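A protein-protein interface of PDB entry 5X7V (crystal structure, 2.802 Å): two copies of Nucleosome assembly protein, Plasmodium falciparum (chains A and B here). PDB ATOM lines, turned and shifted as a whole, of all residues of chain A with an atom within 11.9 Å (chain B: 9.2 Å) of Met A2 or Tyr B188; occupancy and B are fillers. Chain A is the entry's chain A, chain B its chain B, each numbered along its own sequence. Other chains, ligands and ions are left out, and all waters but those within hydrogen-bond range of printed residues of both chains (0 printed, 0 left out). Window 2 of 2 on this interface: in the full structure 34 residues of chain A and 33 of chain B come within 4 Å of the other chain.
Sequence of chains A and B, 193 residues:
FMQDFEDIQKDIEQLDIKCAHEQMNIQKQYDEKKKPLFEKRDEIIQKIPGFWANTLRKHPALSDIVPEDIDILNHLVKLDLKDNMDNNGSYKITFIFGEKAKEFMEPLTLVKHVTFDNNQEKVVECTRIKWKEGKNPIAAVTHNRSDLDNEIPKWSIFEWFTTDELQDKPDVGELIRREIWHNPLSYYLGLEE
OE2 of Glu A13 is in hydrogen-bond range of ND2 of Asn B183 (3.2 Å).
The side-chain hydroxyl of Ser B186 lies within hydrogen-bond range of the backbone carbonyl oxygen of Asn B183, at 3.0 Å.
The backbone carbonyl oxygen of Phe B51 sits at hydrogen-bond distance from the side-chain hydroxyl of Thr B55, at 2.7 Å.
OD1 of Asn B183 lies close to N of Leu B185.
Met A2 touches Leu B185.
Met A2 touches Tyr B188 (CE to CE2, 3.4 Å).
SD of Met A2 touches CD2 of Leu B189, at 3.9 Å.
CB of Asp A4 touches CD1 of Ile B44 (3.0 Å).
Phe A5 touches Ile B44 (N to CD1, 3.6 Å).
Pro B184 touches Phe A5.
CB of Leu B185 touches CE2 of Phe A5, 3.6 Å away.
CG1 of Ile A8 touches CD1 of Ile B44 (3.96 Å).
Asn B183 touches Gln A9 (CG to CG, 3.4 Å).
OE1 of Gln A9 touches CD of Pro B184, 3.7 Å away.
Printed residues of chain B within 4 Å of Met A2: Ile B48, Leu B185, Tyr B188 and Leu B189.
Phe A1 touches none of the printed residues of chain B.
No residue of chain A comes within 4 Å of Pro B49.
No residue of chain A comes within 4 Å of Gly B50.
Printed residues of chain A within 4 Å of Phe B51: Phe A5.
No residue of chain A comes within 4 Å of Asn B54.
No residue of chain A comes within 4 Å of Thr B55.
No residue of chain A comes within 4 Å of Lys B58.
Of chain A, only Phe A5 (3.6 Å) and Gln A9 (3.7 Å) come within 4 Å of Pro B184.
No residue of chain A comes within 4 Å of Ser B186.
Of the printed residues of chain A, Leu B189 touches Met A2.
Of the printed residues of chain B, Phe A5 touches Ile B44 (3.6 Å), Ile B45 (3.5 Å), Phe B51 (3.5 Å), Pro B184 (3.6 Å) and Leu B185 (3.6 Å).
Printed residues of chain A within 4 Å of Asn B183: Gln A9 (3.4 Å) and Glu A13 (3.2 Å).
Printed residues of chain B within 4 Å of Asp A4: Ile B44.
Of the printed residues of chain B, Glu A13 touches Asn B183.
Of the printed residues of chain A, Ile B45 touches Phe A5 (3.5 Å).
Arg B57 touches none of the printed residues of chain A.
The nearest residue of chain A that does not touch Tyr B188 is Phe A5 (6.7 Å).
The nearest printed residue of chain B that does not touch Gln A9 is Leu B185 (5.0 Å).
Of the 12 printed residues of chain A, 7 touch a printed residue of chain B.
Printed residues of chain B that touch a printed residue of chain A: Ile B44, Ile B45, Ile B48, Phe B51, Asn B183, Pro B184, Leu B185, Tyr B188 and Leu B189.
Among the printed residues, 15 pairs touch across the chains.
Among the printed residues, no Asp or Glu carboxylate lies within 4 Å of a Lys or Arg side-chain nitrogen of the other chain.
No position is printed for both chains.
Of the 15 pairs that touch across the chains among the printed residues, none has its exchanged pair printed and touching as well.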
ATOM      1  N   PHE A   1     -11.878 -22.266  -5.027  1.00  0.00           N
ATOM      2  CA  PHE A   1     -10.937 -22.611  -6.103  1.00  0.00           C
ATOM      3  C   PHE A   1      -9.903 -21.523  -6.345  1.00  0.00           C
ATOM      4  O   PHE A   1      -8.740 -21.832  -6.528  1.00  0.00           O
ATOM      5  CB  PHE A   1     -11.652 -22.858  -7.416  1.00  0.00           C
ATOM      6  N   MET A   2     -10.335 -20.269  -6.476  1.00  0.00           N
ATOM      7  CA  MET A   2      -9.454 -19.149  -6.142  1.00  0.00           C
ATOM      8  C   MET A   2      -8.770 -19.419  -4.818  1.00  0.00           C
ATOM      9  O   MET A   2      -7.658 -18.991  -4.604  1.00  0.00           O
ATOM     10  CB  MET A   2     -10.206 -17.835  -6.009  1.00  0.00           C
ATOM     11  CG  MET A   2     -10.530 -17.165  -7.296  1.00  0.00           C
ATOM     12  SD  MET A   2      -9.058 -16.784  -8.250  1.00  0.00           S
ATOM     13  CE  MET A   2      -9.228 -17.966  -9.549  1.00  0.00           C
ATOM     14  N   GLN A   3      -9.464 -20.097  -3.912  1.00  0.00           N
ATOM     15  CA  GLN A   3      -8.905 -20.451  -2.614  1.00  0.00           C
ATOM     16  C   GLN A   3      -7.922 -21.630  -2.713  1.00  0.00           C
ATOM     17  O   GLN A   3      -6.923 -21.672  -2.000  1.00  0.00           O
ATOM     18  CB  GLN A   3     -10.031 -20.783  -1.636  1.00  0.00           C
ATOM     19  CG  GLN A   3      -9.575 -21.364  -0.313  1.00  0.00           C
ATOM     20  CD  GLN A   3      -8.966 -20.324   0.578  1.00  0.00           C
ATOM     21  OE1 GLN A   3      -9.553 -19.253   0.790  1.00  0.00           O
ATOM     22  NE2 GLN A   3      -7.785 -20.625   1.122  1.00  0.00           N
ATOM     23  N   ASP A   4      -8.211 -22.579  -3.598  1.00  0.00           N
ATOM     24  CA  ASP A   4      -7.368 -23.763  -3.739  1.00  0.00           C
ATOM     25  C   ASP A   4      -6.001 -23.391  -4.250  1.00  0.00           C
ATOM     26  O   ASP A   4      -4.995 -24.015  -3.900  1.00  0.00           O
ATOM     27  CB  ASP A   4      -7.996 -24.776  -4.691  1.00  0.00           C
ATOM     28  CG  ASP A   4      -9.192 -25.477  -4.093  1.00  0.00           C
ATOM     29  OD1 ASP A   4      -9.172 -25.744  -2.859  1.00  0.00           O
ATOM     30  OD2 ASP A   4     -10.152 -25.737  -4.872  1.00  0.00           O
ATOM     31  N   PHE A   5      -5.988 -22.362  -5.089  1.00  0.00           N
ATOM     32  CA  PHE A   5      -4.779 -21.909  -5.756  1.00  0.00           C
ATOM     33  C   PHE A   5      -3.887 -21.242  -4.721  1.00  0.00           C
ATOM     34  O   PHE A   5      -2.670 -21.439  -4.710  1.00  0.00           O
ATOM     35  CB  PHE A   5      -5.133 -20.958  -6.905  1.00  0.00           C
ATOM     36  CG  PHE A   5      -4.058 -20.832  -7.948  1.00  0.00           C
ATOM     37  CD1 PHE A   5      -4.329 -21.097  -9.277  1.00  0.00           C
ATOM     38  CD2 PHE A   5      -2.781 -20.446  -7.601  1.00  0.00           C
ATOM     39  CE1 PHE A   5      -3.346 -20.987 -10.229  1.00  0.00           C
ATOM     40  CE2 PHE A   5      -1.792 -20.336  -8.547  1.00  0.00           C
ATOM     41  CZ  PHE A   5      -2.075 -20.604  -9.867  1.00  0.00           C
ATOM     42  N   GLU A   6      -4.510 -20.480  -3.830  1.00  0.00           N
ATOM     43  CA  GLU A   6      -3.793 -19.842  -2.732  1.00  0.00           C
ATOM     44  C   GLU A   6      -3.215 -20.869  -1.759  1.00  0.00           C
ATOM     45  O   GLU A   6      -2.067 -20.736  -1.333  1.00  0.00           O
ATOM     46  CB  GLU A   6      -4.716 -18.861  -2.016  1.00  0.00           C
ATOM     47  CG  GLU A   6      -5.357 -17.914  -2.992  1.00  0.00           C
ATOM     48  CD  GLU A   6      -6.241 -16.872  -2.350  1.00  0.00           C
ATOM     49  OE1 GLU A   6      -6.078 -15.677  -2.677  1.00  0.00           O
ATOM     50  OE2 GLU A   6      -7.120 -17.242  -1.544  1.00  0.00           O
ATOM     51  N   ASP A   7      -4.001 -21.885  -1.417  1.00  0.00           N
ATOM     52  CA  ASP A   7      -3.524 -22.981  -0.572  1.00  0.00           C
ATOM     53  C   ASP A   7      -2.323 -23.689  -1.163  1.00  0.00           C
ATOM     54  O   ASP A   7      -1.385 -24.044  -0.446  1.00  0.00           O
ATOM     55  CB  ASP A   7      -4.612 -24.036  -0.326  1.00  0.00           C
ATOM     56  CG  ASP A   7      -5.640 -23.602   0.698  1.00  0.00           C
ATOM     57  OD1 ASP A   7      -5.414 -22.564   1.377  1.00  0.00           O
ATOM     58  OD2 ASP A   7      -6.652 -24.335   0.850  1.00  0.00           O
ATOM     59  N   ILE A   8      -2.365 -23.932  -2.466  1.00  0.00           N
ATOM     60  CA  ILE A   8      -1.268 -24.637  -3.093  1.00  0.00           C
ATOM     61  C   ILE A   8      -0.041 -23.739  -3.083  1.00  0.00           C
ATOM     62  O   ILE A   8       1.072 -24.200  -2.849  1.00  0.00           O
ATOM     63  CB  ILE A   8      -1.618 -25.099  -4.527  1.00  0.00           C
ATOM     64  CG1 ILE A   8      -2.866 -25.975  -4.476  1.00  0.00           C
ATOM     65  CG2 ILE A   8      -0.469 -25.843  -5.181  1.00  0.00           C
ATOM     66  CD1 ILE A   8      -2.693 -27.199  -3.599  1.00  0.00           C
ATOM     67  N   GLN A   9      -0.255 -22.447  -3.274  1.00  0.00           N
ATOM     68  CA  GLN A   9       0.862 -21.535  -3.394  1.00  0.00           C
ATOM     69  C   GLN A   9       1.473 -21.202  -2.033  1.00  0.00           C
ATOM     70  O   GLN A   9       2.628 -20.788  -1.966  1.00  0.00           O
ATOM     71  CB  GLN A   9       0.435 -20.271  -4.118  1.00  0.00           C
ATOM     72  CG  GLN A   9       1.574 -19.652  -4.845  1.00  0.00           C
ATOM     73  CD  GLN A   9       1.790 -20.263  -6.213  1.00  0.00           C
ATOM     74  OE1 GLN A   9       0.852 -20.407  -6.994  1.00  0.00           O
ATOM     75  NE2 GLN A   9       3.029 -20.633  -6.508  1.00  0.00           N
ATOM     76  N   LYS A  10       0.707 -21.379  -0.958  1.00  0.00           N
ATOM     77  CA  LYS A  10       1.282 -21.379   0.381  1.00  0.00           C
ATOM     78  C   LYS A  10       2.337 -22.473   0.478  1.00  0.00           C
ATOM     79  O   LYS A  10       3.498 -22.197   0.758  1.00  0.00           O
ATOM     80  CB  LYS A  10       0.217 -21.606   1.451  1.00  0.00           C
ATOM     81  CG  LYS A  10      -0.492 -20.366   1.950  1.00  0.00           C
ATOM     82  CD  LYS A  10      -1.578 -20.720   2.963  1.00  0.00           C
ATOM     83  CE  LYS A  10      -2.467 -19.518   3.243  1.00  0.00           C
ATOM     84  NZ  LYS A  10      -3.281 -19.204   2.050  1.00  0.00           N
ATOM     85  N   ASP A  11       1.910 -23.716   0.242  1.00  0.00           N
ATOM     86  CA  ASP A  11       2.786 -24.889   0.207  1.00  0.00           C
ATOM     87  C   ASP A  11       4.037 -24.767  -0.706  1.00  0.00           C
ATOM     88  O   ASP A  11       5.122 -25.219  -0.354  1.00  0.00           O
ATOM     89  CB  ASP A  11       1.964 -26.104  -0.221  1.00  0.00           C
ATOM     90  CG  ASP A  11       0.766 -26.348   0.684  1.00  0.00           C
ATOM     91  OD1 ASP A  11       0.804 -25.903   1.855  1.00  0.00           O
ATOM     92  OD2 ASP A  11      -0.206 -27.007   0.239  1.00  0.00           O
ATOM     93  N   GLU A  13       5.469 -21.811  -1.625  1.00  0.00           N
ATOM     94  CA  GLU A  13       6.346 -20.777  -1.066  1.00  0.00           C
ATOM     95  C   GLU A  13       7.074 -21.245   0.184  1.00  0.00           C
ATOM     96  O   GLU A  13       8.253 -20.963   0.343  1.00  0.00           O
ATOM     97  CB  GLU A  13       5.570 -19.491  -0.783  1.00  0.00           C
ATOM     98  CG  GLU A  13       5.427 -18.626  -2.049  1.00  0.00           C
ATOM     99  CD  GLU A  13       4.602 -17.366  -1.837  1.00  0.00           C
ATOM    100  OE1 GLU A  13       5.138 -16.413  -1.224  1.00  0.00           O
ATOM    101  OE2 GLU A  13       3.428 -17.324  -2.293  1.00  0.00           O
ATOM    102  N   ILE B  44      -5.563 -27.419 -10.861  1.00  0.00           N
ATOM    103  CA  ILE B  44      -6.456 -26.330 -10.512  1.00  0.00           C
ATOM    104  C   ILE B  44      -6.666 -25.312 -11.611  1.00  0.00           C
ATOM    105  O   ILE B  44      -7.748 -24.818 -11.785  1.00  0.00           O
ATOM    106  CB  ILE B  44      -5.924 -25.531  -9.338  1.00  0.00           C
ATOM    107  CG1 ILE B  44      -5.954 -26.348  -8.075  1.00  0.00           C
ATOM    108  CG2 ILE B  44      -6.774 -24.310  -9.126  1.00  0.00           C
ATOM    109  CD1 ILE B  44      -6.015 -25.504  -6.829  1.00  0.00           C
ATOM    110  N   ILE B  45      -5.612 -24.980 -12.327  1.00  0.00           N
ATOM    111  CA  ILE B  45      -5.700 -23.958 -13.334  1.00  0.00           C
ATOM    112  C   ILE B  45      -6.701 -24.338 -14.372  1.00  0.00           C
ATOM    113  O   ILE B  45      -7.477 -23.528 -14.820  1.00  0.00           O
ATOM    114  CB  ILE B  45      -4.359 -23.761 -14.000  1.00  0.00           C
ATOM    115  CG1 ILE B  45      -3.475 -22.915 -13.125  1.00  0.00           C
ATOM    116  CG2 ILE B  45      -4.522 -23.080 -15.332  1.00  0.00           C
ATOM    117  CD1 ILE B  45      -2.132 -22.685 -13.748  1.00  0.00           C
ATOM    118  N   LYS B  47      -9.377 -25.443 -14.127  1.00  0.00           N
ATOM    119  CA  LYS B  47     -10.754 -25.095 -13.737  1.00  0.00           C
ATOM    120  C   LYS B  47     -10.977 -23.570 -13.620  1.00  0.00           C
ATOM    121  O   LYS B  47     -12.093 -23.152 -13.283  1.00  0.00           O
ATOM    122  CB  LYS B  47     -11.159 -25.767 -12.417  1.00  0.00           C
ATOM    123  CG  LYS B  47     -11.223 -27.320 -12.379  1.00  0.00           C
ATOM    124  CD  LYS B  47     -12.550 -27.961 -12.829  1.00  0.00           C
ATOM    125  CE  LYS B  47     -13.617 -28.024 -11.708  1.00  0.00           C
ATOM    126  NZ  LYS B  47     -14.900 -28.681 -12.146  1.00  0.00           N
ATOM    127  N   ILE B  48     -10.021 -22.781 -14.100  1.00  0.00           N
ATOM    128  CA  ILE B  48     -10.165 -21.329 -14.157  1.00  0.00           C
ATOM    129  C   ILE B  48     -10.102 -20.942 -15.643  1.00  0.00           C
ATOM    130  O   ILE B  48      -9.010 -20.803 -16.194  1.00  0.00           O
ATOM    131  CB  ILE B  48      -9.043 -20.611 -13.388  1.00  0.00           C
ATOM    132  CG1 ILE B  48      -9.307 -20.668 -11.882  1.00  0.00           C
ATOM    133  CG2 ILE B  48      -8.913 -19.171 -13.857  1.00  0.00           C
ATOM    134  CD1 ILE B  48      -8.060 -20.534 -11.038  1.00  0.00           C
ATOM    135  N   PRO B  49     -11.256 -20.769 -16.297  1.00  0.00           N
ATOM    136  CA  PRO B  49     -11.263 -20.457 -17.724  1.00  0.00           C
ATOM    137  C   PRO B  49     -10.261 -19.363 -18.130  1.00  0.00           C
ATOM    138  O   PRO B  49     -10.285 -18.255 -17.588  1.00  0.00           O
ATOM    139  CB  PRO B  49     -12.696 -19.986 -17.961  1.00  0.00           C
ATOM    140  CG  PRO B  49     -13.219 -19.649 -16.575  1.00  0.00           C
ATOM    141  CD  PRO B  49     -12.567 -20.571 -15.662  1.00  0.00           C
ATOM    142  N   GLY B  50      -9.380 -19.698 -19.071  1.00  0.00           N
ATOM    143  CA  GLY B  50      -8.447 -18.745 -19.631  1.00  0.00           C
ATOM    144  C   GLY B  50      -7.515 -18.099 -18.629  1.00  0.00           C
ATOM    145  O   GLY B  50      -7.220 -16.908 -18.736  1.00  0.00           O
ATOM    146  N   PHE B  51      -7.050 -18.888 -17.665  1.00  0.00           N
ATOM    147  CA  PHE B  51      -6.151 -18.406 -16.633  1.00  0.00           C
ATOM    148  C   PHE B  51      -4.891 -17.759 -17.208  1.00  0.00           C
ATOM    149  O   PHE B  51      -4.651 -16.566 -17.014  1.00  0.00           O
ATOM    150  CB  PHE B  51      -5.770 -19.552 -15.691  1.00  0.00           C
ATOM    151  CG  PHE B  51      -4.824 -19.143 -14.598  1.00  0.00           C
ATOM    152  CD1 PHE B  51      -5.277 -18.409 -13.527  1.00  0.00           C
ATOM    153  CD2 PHE B  51      -3.482 -19.489 -14.650  1.00  0.00           C
ATOM    154  CE1 PHE B  51      -4.415 -18.018 -12.530  1.00  0.00           C
ATOM    155  CE2 PHE B  51      -2.610 -19.098 -13.663  1.00  0.00           C
ATOM    156  CZ  PHE B  51      -3.071 -18.364 -12.599  1.00  0.00           C
ATOM    157  N   TRP B  52      -4.083 -18.552 -17.895  1.00  0.00           N
ATOM    158  CA  TRP B  52      -2.830 -18.066 -18.431  1.00  0.00           C
ATOM    159  C   TRP B  52      -3.004 -16.890 -19.373  1.00  0.00           C
ATOM    160  O   TRP B  52      -2.206 -15.939 -19.348  1.00  0.00           O
ATOM    161  CB  TRP B  52      -2.095 -19.195 -19.152  1.00  0.00           C
ATOM    162  CG  TRP B  52      -1.450 -20.163 -18.217  1.00  0.00           C
ATOM    163  CD1 TRP B  52      -1.689 -21.498 -18.122  1.00  0.00           C
ATOM    164  CD2 TRP B  52      -0.460 -19.860 -17.229  1.00  0.00           C
ATOM    165  NE1 TRP B  52      -0.905 -22.048 -17.141  1.00  0.00           N
ATOM    166  CE2 TRP B  52      -0.140 -21.062 -16.582  1.00  0.00           C
ATOM    167  CE3 TRP B  52       0.183 -18.688 -16.833  1.00  0.00           C
ATOM    168  CZ2 TRP B  52       0.801 -21.128 -15.566  1.00  0.00           C
ATOM    169  CZ3 TRP B  52       1.112 -18.757 -15.820  1.00  0.00           C
ATOM    170  CH2 TRP B  52       1.409 -19.966 -15.195  1.00  0.00           C
ATOM    171  N   ALA B  53      -4.041 -16.954 -20.207  1.00  0.00           N
ATOM    172  CA  ALA B  53      -4.303 -15.899 -21.191  1.00  0.00           C
ATOM    173  C   ALA B  53      -4.465 -14.534 -20.538  1.00  0.00           C
ATOM    174  O   ALA B  53      -4.232 -13.532 -21.141  1.00  0.00           O
ATOM    175  CB  ALA B  53      -5.544 -16.232 -22.005  1.00  0.00           C
ATOM    176  N   ASN B  54      -4.809 -14.542 -19.267  1.00  0.00           N
ATOM    177  CA  ASN B  54      -5.300 -13.406 -18.493  1.00  0.00           C
ATOM    178  C   ASN B  54      -4.294 -12.987 -17.453  1.00  0.00           C
ATOM    179  O   ASN B  54      -4.231 -11.834 -17.059  1.00  0.00           O
ATOM    180  CB  ASN B  54      -6.661 -13.818 -17.948  1.00  0.00           C
ATOM    181  CG  ASN B  54      -7.773 -13.413 -18.876  1.00  0.00           C
ATOM    182  OD1 ASN B  54      -7.811 -13.789 -20.050  1.00  0.00           O
ATOM    183  ND2 ASN B  54      -8.832 -12.993 -18.248  1.00  0.00           N
ATOM    184  N   THR B  55      -3.460 -13.944 -17.088  1.00  0.00           N
ATOM    185  CA  THR B  55      -2.338 -13.766 -16.194  1.00  0.00           C
ATOM    186  C   THR B  55      -1.156 -13.065 -16.844  1.00  0.00           C
ATOM    187  O   THR B  55      -0.591 -12.121 -16.285  1.00  0.00           O
ATOM    188  CB  THR B  55      -1.883 -15.132 -15.700  1.00  0.00           C
ATOM    189  OG1 THR B  55      -2.991 -15.784 -15.056  1.00  0.00           O
ATOM    190  CG2 THR B  55      -0.695 -15.013 -14.746  1.00  0.00           C
ATOM    191  N   LEU B  56      -0.784 -13.527 -18.031  1.00  0.00           N
ATOM    192  CA  LEU B  56       0.355 -12.954 -18.737  1.00  0.00           C
ATOM    193  C   LEU B  56       0.098 -11.487 -19.049  1.00  0.00           C
ATOM    194  O   LEU B  56       0.857 -10.637 -18.634  1.00  0.00           O
ATOM    195  CB  LEU B  56       0.673 -13.739 -20.024  1.00  0.00           C
ATOM    196  CG  LEU B  56       1.074 -15.203 -19.791  1.00  0.00           C
ATOM    197  CD1 LEU B  56       0.995 -16.058 -21.054  1.00  0.00           C
ATOM    198  CD2 LEU B  56       2.464 -15.281 -19.172  1.00  0.00           C
ATOM    199  N   ARG B  57      -0.981 -11.163 -19.747  1.00  0.00           N
ATOM    200  CA  ARG B  57      -1.137  -9.784 -20.204  1.00  0.00           C
ATOM    201  C   ARG B  57      -1.365  -8.776 -19.067  1.00  0.00           C
ATOM    202  O   ARG B  57      -1.264  -7.572 -19.311  1.00  0.00           O
ATOM    203  CB  ARG B  57      -2.256  -9.689 -21.252  1.00  0.00           C
ATOM    204  CG  ARG B  57      -3.511 -10.457 -20.930  1.00  0.00           C
ATOM    205  CD  ARG B  57      -4.693  -9.918 -21.740  1.00  0.00           C
ATOM    206  NE  ARG B  57      -5.975 -10.144 -21.080  1.00  0.00           N
ATOM    207  CZ  ARG B  57      -7.101  -9.529 -21.415  1.00  0.00           C
ATOM    208  NH1 ARG B  57      -7.102  -8.632 -22.388  1.00  0.00           N
ATOM    209  NH2 ARG B  57      -8.220  -9.802 -20.762  1.00  0.00           N
ATOM    210  N   LYS B  58      -1.641  -9.236 -17.845  1.00  0.00           N
ATOM    211  CA  LYS B  58      -1.722  -8.303 -16.721  1.00  0.00           C
ATOM    212  C   LYS B  58      -0.338  -7.921 -16.231  1.00  0.00           C
ATOM    213  O   LYS B  58      -0.208  -7.058 -15.364  1.00  0.00           O
ATOM    214  CB  LYS B  58      -2.538  -8.873 -15.555  1.00  0.00           C
ATOM    215  CG  LYS B  58      -4.006  -8.430 -15.521  1.00  0.00           C
ATOM    216  CD  LYS B  58      -4.909  -9.467 -14.845  1.00  0.00           C
ATOM    217  CE  LYS B  58      -5.312  -9.033 -13.434  1.00  0.00           C
ATOM    218  NZ  LYS B  58      -6.204  -7.831 -13.389  1.00  0.00           N
ATOM    219  N   HIS B  59       0.687  -8.504 -16.847  1.00  0.00           N
ATOM    220  CA  HIS B  59       2.065  -8.148 -16.551  1.00  0.00           C
ATOM    221  C   HIS B  59       2.281  -6.928 -17.443  1.00  0.00           C
ATOM    222  O   HIS B  59       2.027  -6.991 -18.645  1.00  0.00           O
ATOM    223  CB  HIS B  59       3.018  -9.275 -16.940  1.00  0.00           C
ATOM    224  CG  HIS B  59       4.452  -8.993 -16.620  1.00  0.00           C
ATOM    225  ND1 HIS B  59       5.494  -9.695 -17.186  1.00  0.00           N
ATOM    226  CD2 HIS B  59       5.018  -8.085 -15.790  1.00  0.00           C
ATOM    227  CE1 HIS B  59       6.640  -9.231 -16.720  1.00  0.00           C
ATOM    228  NE2 HIS B  59       6.379  -8.254 -15.871  1.00  0.00           N
ATOM    229  N   ILE B 180       6.843 -14.283 -12.998  1.00  0.00           N
ATOM    230  CA  ILE B 180       5.474 -14.797 -13.004  1.00  0.00           C
ATOM    231  C   ILE B 180       5.377 -16.175 -12.383  1.00  0.00           C
ATOM    232  O   ILE B 180       4.714 -16.356 -11.354  1.00  0.00           O
ATOM    233  CB  ILE B 180       4.868 -14.859 -14.424  1.00  0.00           C
ATOM    234  CG1 ILE B 180       4.700 -13.447 -15.000  1.00  0.00           C
ATOM    235  CG2 ILE B 180       3.507 -15.562 -14.384  1.00  0.00           C
ATOM    236  CD1 ILE B 180       4.288 -13.430 -16.455  1.00  0.00           C
ATOM    237  N   ASN B 183       4.747 -17.493  -8.607  1.00  0.00           N
ATOM    238  CA  ASN B 183       3.386 -17.299  -8.121  1.00  0.00           C
ATOM    239  C   ASN B 183       2.548 -16.535  -9.119  1.00  0.00           C
ATOM    240  O   ASN B 183       2.419 -15.321  -9.009  1.00  0.00           O
ATOM    241  CB  ASN B 183       3.361 -16.566  -6.782  1.00  0.00           C
ATOM    242  CG  ASN B 183       1.968 -16.566  -6.134  1.00  0.00           C
ATOM    243  OD1 ASN B 183       0.963 -16.849  -6.776  1.00  0.00           O
ATOM    244  ND2 ASN B 183       1.917 -16.240  -4.855  1.00  0.00           N
ATOM    245  N   PRO B 184       1.927 -17.260 -10.069  1.00  0.00           N
ATOM    246  CA  PRO B 184       1.191 -16.646 -11.169  1.00  0.00           C
ATOM    247  C   PRO B 184      -0.122 -16.006 -10.733  1.00  0.00           C
ATOM    248  O   PRO B 184      -0.575 -15.057 -11.371  1.00  0.00           O
ATOM    249  CB  PRO B 184       0.945 -17.824 -12.109  1.00  0.00           C
ATOM    250  CG  PRO B 184       0.861 -18.969 -11.224  1.00  0.00           C
ATOM    251  CD  PRO B 184       1.822 -18.731 -10.108  1.00  0.00           C
ATOM    252  N   LEU B 185      -0.718 -16.515  -9.662  1.00  0.00           N
ATOM    253  CA  LEU B 185      -2.017 -16.033  -9.192  1.00  0.00           C
ATOM    254  C   LEU B 185      -1.947 -14.568  -8.774  1.00  0.00           C
ATOM    255  O   LEU B 185      -2.944 -13.846  -8.882  1.00  0.00           O
ATOM    256  CB  LEU B 185      -2.538 -16.892  -8.032  1.00  0.00           C
ATOM    257  CG  LEU B 185      -3.874 -16.458  -7.432  1.00  0.00           C
ATOM    258  CD1 LEU B 185      -5.085 -17.136  -8.062  1.00  0.00           C
ATOM    259  CD2 LEU B 185      -3.831 -16.684  -5.944  1.00  0.00           C
ATOM    260  N   SER B 186      -0.774 -14.149  -8.299  1.00  0.00           N
ATOM    261  CA  SER B 186      -0.449 -12.735  -8.102  1.00  0.00           C
ATOM    262  C   SER B 186      -0.954 -11.909  -9.284  1.00  0.00           C
ATOM    263  O   SER B 186      -1.677 -10.926  -9.124  1.00  0.00           O
ATOM    264  CB  SER B 186       1.067 -12.549  -7.956  1.00  0.00           C
ATOM    265  OG  SER B 186       1.608 -13.309  -6.874  1.00  0.00           O
ATOM    266  N   TYR B 187      -0.592 -12.341 -10.485  1.00  0.00           N
ATOM    267  CA  TYR B 187      -0.930 -11.588 -11.678  1.00  0.00           C
ATOM    268  C   TYR B 187      -2.365 -11.807 -12.129  1.00  0.00           C
ATOM    269  O   TYR B 187      -2.933 -10.946 -12.784  1.00  0.00           O
ATOM    270  CB  TYR B 187       0.038 -11.929 -12.819  1.00  0.00           C
ATOM    271  CG  TYR B 187       1.427 -11.372 -12.602  1.00  0.00           C
ATOM    272  CD1 TYR B 187       1.743 -10.075 -12.992  1.00  0.00           C
ATOM    273  CD2 TYR B 187       2.418 -12.139 -11.996  1.00  0.00           C
ATOM    274  CE1 TYR B 187       3.008  -9.556 -12.791  1.00  0.00           C
ATOM    275  CE2 TYR B 187       3.688 -11.633 -11.785  1.00  0.00           C
ATOM    276  CZ  TYR B 187       3.984 -10.340 -12.181  1.00  0.00           C
ATOM    277  OH  TYR B 187       5.260  -9.835 -11.965  1.00  0.00           O
ATOM    278  N   TYR B 188      -2.955 -12.948 -11.799  1.00  0.00           N
ATOM    279  CA  TYR B 188      -4.336 -13.188 -12.185  1.00  0.00           C
ATOM    280  C   TYR B 188      -5.277 -12.220 -11.457  1.00  0.00           C
ATOM    281  O   TYR B 188      -6.224 -11.697 -12.045  1.00  0.00           O
ATOM    282  CB  TYR B 188      -4.738 -14.646 -11.905  1.00  0.00           C
ATOM    283  CG  TYR B 188      -6.154 -14.994 -12.365  1.00  0.00           C
ATOM    284  CD1 TYR B 188      -6.465 -15.050 -13.717  1.00  0.00           C
ATOM    285  CD2 TYR B 188      -7.164 -15.265 -11.449  1.00  0.00           C
ATOM    286  CE1 TYR B 188      -7.718 -15.353 -14.134  1.00  0.00           C
ATOM    287  CE2 TYR B 188      -8.421 -15.570 -11.864  1.00  0.00           C
ATOM    288  CZ  TYR B 188      -8.696 -15.611 -13.206  1.00  0.00           C
ATOM    289  OH  TYR B 188      -9.962 -15.903 -13.648  1.00  0.00           O
ATOM    290  N   LEU B 189      -4.987 -11.976 -10.180  1.00  0.00           N
ATOM    291  CA  LEU B 189      -5.799 -11.108  -9.323  1.00  0.00           C
ATOM    292  C   LEU B 189      -5.467  -9.618  -9.488  1.00  0.00           C
ATOM    293  O   LEU B 189      -4.340  -9.179  -9.213  1.00  0.00           O
ATOM    294  CB  LEU B 189      -5.629 -11.519  -7.850  1.00  0.00           C
ATOM    295  CG  LEU B 189      -5.976 -12.985  -7.563  1.00  0.00           C
ATOM    296  CD1 LEU B 189      -5.673 -13.374  -6.142  1.00  0.00           C
ATOM    297  CD2 LEU B 189      -7.417 -13.257  -7.894  1.00  0.00           C
